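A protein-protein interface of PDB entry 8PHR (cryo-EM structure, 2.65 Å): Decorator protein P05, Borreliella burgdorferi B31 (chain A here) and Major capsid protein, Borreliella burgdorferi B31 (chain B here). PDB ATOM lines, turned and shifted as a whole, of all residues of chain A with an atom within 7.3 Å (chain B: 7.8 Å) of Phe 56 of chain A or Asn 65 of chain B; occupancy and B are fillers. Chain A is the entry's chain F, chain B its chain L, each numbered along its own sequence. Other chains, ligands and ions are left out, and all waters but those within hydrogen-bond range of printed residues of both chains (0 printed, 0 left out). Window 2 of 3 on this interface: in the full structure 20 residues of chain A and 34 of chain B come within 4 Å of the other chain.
O of Ile 67 of chain B lies within hydrogen-bond range of N of Thr 53 of chain A, 3.2 Å away.
The side-chain hydroxyl (OG) of Ser 54 of chain A sits close to the backbone NH (N) of Phe 56 of chain A.
N of Ser 54 of chain A sits at hydrogen-bond distance from OD2 of Asp 57 of chain A.
Asn 65 of chain B touches Thr 53 of chain A (O to O, 3.98 Å).
Thr 66 of chain B touches Thr 53 of chain A (CG2 to N, 3.7 Å).
Asn 65 of chain B touches Ser 54 of chain A.
Thr 66 of chain B touches Ser 54 of chain A.
Asn 65 of chain B touches Lys 55 of chain A (O to N, 3.7 Å).
Phe 56 of chain A touches Asn 65 of chain B (CE2 to ND2, 3.3 Å).
Phe 56 of chain A touches one residue of chain B.
Of chain A, only Thr 53 (3.98 Å), Ser 54 (3.5 Å), Lys 55 (3.7 Å) and Phe 56 (3.3 Å) come within 4 Å of Asn 65 of chain B.
Printed residues of chain A within 4 Å of Ile 67 of chain B: Thr 53.
Printed residues of chain A within 4 Å of Thr 66 of chain B: Thr 53 and Ser 54.
Of the printed residues of chain B, Thr 53 of chain A touches Asn 65 (3.98 Å), Thr 66 (3.7 Å) and Ile 67 (3.2 Å).
Of the printed residues of chain B, Lys 55 of chain A touches Asn 65 (3.7 Å).
Of the printed residues of chain B, Ser 54 of chain A touches Asn 65 and Thr 66.
The nearest printed residue of chain A that does not touch Asn 65 of chain B is Asp 57 of chain A (7.7 Å).
Of the 8 printed residues of chain A, 4 touch a printed residue of chain B.
Printed residues of chain A that touch a printed residue of chain B: Thr 53, Ser 54, Lys 55 and Phe 56.
Of the 9 printed residues of chain B, 3 touch a printed residue of chain A.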
ATOM      1  N   THR A  53       0.226 -29.941  -6.546  1.00  0.00           N
ATOM      2  CA  THR A  53       0.792 -30.071  -5.211  1.00  0.00           C
ATOM      3  C   THR A  53      -0.113 -29.387  -4.199  1.00  0.00           C
ATOM      4  O   THR A  53      -0.637 -28.298  -4.456  1.00  0.00           O
ATOM      5  CB  THR A  53       2.203 -29.466  -5.146  1.00  0.00           C
ATOM      6  OG1 THR A  53       3.021 -30.043  -6.171  1.00  0.00           O
ATOM      7  CG2 THR A  53       2.843 -29.733  -3.791  1.00  0.00           C
ATOM      8  N   SER A  54      -0.295 -30.030  -3.051  1.00  0.00           N
ATOM      9  CA  SER A  54      -1.084 -29.486  -1.958  1.00  0.00           C
ATOM     10  C   SER A  54      -0.178 -28.807  -0.938  1.00  0.00           C
ATOM     11  O   SER A  54       0.998 -29.152  -0.797  1.00  0.00           O
ATOM     12  CB  SER A  54      -1.905 -30.583  -1.277  1.00  0.00           C
ATOM     13  OG  SER A  54      -2.345 -30.170   0.006  1.00  0.00           O
ATOM     14  N   LYS A  55      -0.743 -27.828  -0.228  1.00  0.00           N
ATOM     15  CA  LYS A  55       0.025 -27.099   0.775  1.00  0.00           C
ATOM     16  C   LYS A  55       0.438 -27.999   1.933  1.00  0.00           C
ATOM     17  O   LYS A  55       1.492 -27.782   2.545  1.00  0.00           O
ATOM     18  CB  LYS A  55      -0.788 -25.906   1.285  1.00  0.00           C
ATOM     19  CG  LYS A  55      -0.167 -25.172   2.463  1.00  0.00           C
ATOM     20  CD  LYS A  55      -1.113 -24.125   3.027  1.00  0.00           C
ATOM     21  CE  LYS A  55      -0.500 -23.419   4.226  1.00  0.00           C
ATOM     22  NZ  LYS A  55      -1.405 -22.376   4.780  1.00  0.00           N
ATOM     23  N   PHE A  56      -0.357 -29.023   2.235  1.00  0.00           N
ATOM     24  CA  PHE A  56      -0.136 -29.883   3.395  1.00  0.00           C
ATOM     25  C   PHE A  56       0.506 -31.211   3.012  1.00  0.00           C
ATOM     26  O   PHE A  56       0.198 -32.254   3.596  1.00  0.00           O
ATOM     27  CB  PHE A  56      -1.451 -30.115   4.133  1.00  0.00           C
ATOM     28  CG  PHE A  56      -2.211 -28.852   4.421  1.00  0.00           C
ATOM     29  CD1 PHE A  56      -1.654 -27.857   5.207  1.00  0.00           C
ATOM     30  CD2 PHE A  56      -3.477 -28.655   3.897  1.00  0.00           C
ATOM     31  CE1 PHE A  56      -2.349 -26.692   5.472  1.00  0.00           C
ATOM     32  CE2 PHE A  56      -4.178 -27.493   4.158  1.00  0.00           C
ATOM     33  CZ  PHE A  56      -3.613 -26.510   4.946  1.00  0.00           C
ATOM     34  N   ASP A  57       1.406 -31.199   2.031  1.00  0.00           N
ATOM     35  CA  ASP A  57       2.127 -32.397   1.626  1.00  0.00           C
ATOM     36  C   ASP A  57       3.373 -32.575   2.484  1.00  0.00           C
ATOM     37  O   ASP A  57       4.044 -31.601   2.839  1.00  0.00           O
ATOM     38  CB  ASP A  57       2.514 -32.321   0.148  1.00  0.00           C
ATOM     39  CG  ASP A  57       1.442 -32.883  -0.764  1.00  0.00           C
ATOM     40  OD1 ASP A  57       0.447 -33.431  -0.246  1.00  0.00           O
ATOM     41  OD2 ASP A  57       1.595 -32.779  -1.999  1.00  0.00           O
ATOM     42  N   LYS A  58       3.677 -33.827   2.816  1.00  0.00           N
ATOM     43  CA  LYS A  58       4.810 -34.152   3.672  1.00  0.00           C
ATOM     44  C   LYS A  58       6.037 -34.439   2.812  1.00  0.00           C
ATOM     45  O   LYS A  58       5.996 -35.307   1.934  1.00  0.00           O
ATOM     46  CB  LYS A  58       4.483 -35.350   4.564  1.00  0.00           C
ATOM     47  CG  LYS A  58       5.452 -35.552   5.716  1.00  0.00           C
ATOM     48  CD  LYS A  58       5.162 -36.846   6.460  1.00  0.00           C
ATOM     49  CE  LYS A  58       5.775 -36.833   7.851  1.00  0.00           C
ATOM     50  NZ  LYS A  58       7.215 -36.455   7.819  1.00  0.00           N
ATOM     51  N   LEU A  59       7.121 -33.710   3.067  1.00  0.00           N
ATOM     52  CA  LEU A  59       8.378 -33.867   2.346  1.00  0.00           C
ATOM     53  C   LEU A  59       9.491 -34.131   3.349  1.00  0.00           C
ATOM     54  O   LEU A  59       9.606 -33.418   4.350  1.00  0.00           O
ATOM     55  CB  LEU A  59       8.700 -32.617   1.522  1.00  0.00           C
ATOM     56  CG  LEU A  59       7.652 -32.156   0.509  1.00  0.00           C
ATOM     57  CD1 LEU A  59       8.118 -30.904  -0.217  1.00  0.00           C
ATOM     58  CD2 LEU A  59       7.343 -33.262  -0.479  1.00  0.00           C
ATOM     59  N   ASN A 120       1.571 -40.566   1.507  1.00  0.00           N
ATOM     60  CA  ASN A 120       0.965 -39.438   0.820  1.00  0.00           C
ATOM     61  C   ASN A 120       0.740 -39.774  -0.649  1.00  0.00           C
ATOM     62  O   ASN A 120       1.361 -40.684  -1.207  1.00  0.00           O
ATOM     63  CB  ASN A 120       1.847 -38.191   0.948  1.00  0.00           C
ATOM     64  CG  ASN A 120       1.062 -36.904   0.806  1.00  0.00           C
ATOM     65  OD1 ASN A 120      -0.136 -36.922   0.526  1.00  0.00           O
ATOM     66  ND2 ASN A 120       1.734 -35.777   1.002  1.00  0.00           N
ATOM     67  N   THR B  58      -7.083 -25.287 -12.085  1.00  0.00           N
ATOM     68  CA  THR B  58      -7.919 -25.844 -11.033  1.00  0.00           C
ATOM     69  C   THR B  58      -9.052 -24.874 -10.725  1.00  0.00           C
ATOM     70  O   THR B  58      -8.807 -23.694 -10.456  1.00  0.00           O
ATOM     71  CB  THR B  58      -7.099 -26.121  -9.769  1.00  0.00           C
ATOM     72  OG1 THR B  58      -6.241 -27.246  -9.990  1.00  0.00           O
ATOM     73  CG2 THR B  58      -8.013 -26.408  -8.588  1.00  0.00           C
ATOM     74  N   ILE B  60     -11.752 -23.052  -8.591  1.00  0.00           N
ATOM     75  CA  ILE B  60     -11.880 -22.680  -7.181  1.00  0.00           C
ATOM     76  C   ILE B  60     -13.363 -22.798  -6.837  1.00  0.00           C
ATOM     77  O   ILE B  60     -14.135 -21.846  -6.959  1.00  0.00           O
ATOM     78  CB  ILE B  60     -11.320 -21.287  -6.900  1.00  0.00           C
ATOM     79  CG1 ILE B  60      -9.841 -21.227  -7.282  1.00  0.00           C
ATOM     80  CG2 ILE B  60     -11.494 -20.927  -5.432  1.00  0.00           C
ATOM     81  CD1 ILE B  60      -9.009 -22.331  -6.662  1.00  0.00           C
ATOM     82  N   ASN B  62     -15.879 -24.452  -3.696  1.00  0.00           N
ATOM     83  CA  ASN B  62     -15.975 -25.002  -2.336  1.00  0.00           C
ATOM     84  C   ASN B  62     -14.576 -24.952  -1.722  1.00  0.00           C
ATOM     85  O   ASN B  62     -13.944 -23.884  -1.746  1.00  0.00           O
ATOM     86  CB  ASN B  62     -16.627 -26.380  -2.387  1.00  0.00           C
ATOM     87  CG  ASN B  62     -18.111 -26.311  -2.682  1.00  0.00           C
ATOM     88  OD1 ASN B  62     -18.705 -25.233  -2.689  1.00  0.00           O
ATOM     89  ND2 ASN B  62     -18.720 -27.465  -2.930  1.00  0.00           N
ATOM     90  N   GLU B  63     -14.060 -26.047  -1.175  1.00  0.00           N
ATOM     91  CA  GLU B  63     -12.749 -26.078  -0.544  1.00  0.00           C
ATOM     92  C   GLU B  63     -11.817 -26.988  -1.331  1.00  0.00           C
ATOM     93  O   GLU B  63     -12.204 -28.088  -1.738  1.00  0.00           O
ATOM     94  CB  GLU B  63     -12.850 -26.562   0.904  1.00  0.00           C
ATOM     95  CG  GLU B  63     -13.809 -25.764   1.768  1.00  0.00           C
ATOM     96  CD  GLU B  63     -14.065 -26.426   3.109  1.00  0.00           C
ATOM     97  OE1 GLU B  63     -13.503 -27.514   3.351  1.00  0.00           O
ATOM     98  OE2 GLU B  63     -14.829 -25.861   3.918  1.00  0.00           O
ATOM     99  N   VAL B  64     -10.586 -26.526  -1.546  1.00  0.00           N
ATOM    100  CA  VAL B  64      -9.584 -27.298  -2.272  1.00  0.00           C
ATOM    101  C   VAL B  64      -8.207 -26.932  -1.736  1.00  0.00           C
ATOM    102  O   VAL B  64      -7.955 -25.790  -1.344  1.00  0.00           O
ATOM    103  CB  VAL B  64      -9.680 -27.061  -3.799  1.00  0.00           C
ATOM    104  CG1 VAL B  64      -9.440 -25.595  -4.137  1.00  0.00           C
ATOM    105  CG2 VAL B  64      -8.706 -27.961  -4.551  1.00  0.00           C
ATOM    106  N   ASN B  65      -7.316 -27.921  -1.708  1.00  0.00           N
ATOM    107  CA  ASN B  65      -5.945 -27.735  -1.255  1.00  0.00           C
ATOM    108  C   ASN B  65      -4.902 -27.966  -2.338  1.00  0.00           C
ATOM    109  O   ASN B  65      -3.826 -27.367  -2.272  1.00  0.00           O
ATOM    110  CB  ASN B  65      -5.642 -28.671  -0.073  1.00  0.00           C
ATOM    111  CG  ASN B  65      -6.209 -28.160   1.235  1.00  0.00           C
ATOM    112  OD1 ASN B  65      -6.517 -26.977   1.371  1.00  0.00           O
ATOM    113  ND2 ASN B  65      -6.354 -29.053   2.207  1.00  0.00           N
ATOM    114  N   THR B  66      -5.187 -28.811  -3.325  1.00  0.00           N
ATOM    115  CA  THR B  66      -4.229 -29.140  -4.374  1.00  0.00           C
ATOM    116  C   THR B  66      -4.489 -28.264  -5.595  1.00  0.00           C
ATOM    117  O   THR B  66      -5.589 -28.285  -6.158  1.00  0.00           O
ATOM    118  CB  THR B  66      -4.324 -30.618  -4.743  1.00  0.00           C
ATOM    119  OG1 THR B  66      -4.295 -31.412  -3.550  1.00  0.00           O
ATOM    120  CG2 THR B  66      -3.162 -31.018  -5.634  1.00  0.00           C
ATOM    121  N   ILE B  67      -3.476 -27.498  -6.003  1.00  0.00           N
ATOM    122  CA  ILE B  67      -3.586 -26.571  -7.121  1.00  0.00           C
ATOM    123  C   ILE B  67      -2.538 -26.935  -8.167  1.00  0.00           C
ATOM    124  O   ILE B  67      -1.524 -27.574  -7.874  1.00  0.00           O
ATOM    125  CB  ILE B  67      -3.423 -25.102  -6.671  1.00  0.00           C
ATOM    126  CG1 ILE B  67      -4.154 -24.857  -5.350  1.00  0.00           C
ATOM    127  CG2 ILE B  67      -3.962 -24.144  -7.724  1.00  0.00           C
ATOM    128  CD1 ILE B  67      -5.658 -25.013  -5.443  1.00  0.00           C
ATOM    129  N   SER B  68      -2.799 -26.522  -9.406  1.00  0.00           N
ATOM    130  CA  SER B  68      -1.848 -26.717 -10.490  1.00  0.00           C
ATOM    131  C   SER B  68      -0.615 -25.839 -10.282  1.00  0.00           C
ATOM    132  O   SER B  68      -0.664 -24.801  -9.616  1.00  0.00           O
ATOM    133  CB  SER B  68      -2.497 -26.402 -11.838  1.00  0.00           C
ATOM    134  OG  SER B  68      -3.525 -27.330 -12.138  1.00  0.00           O
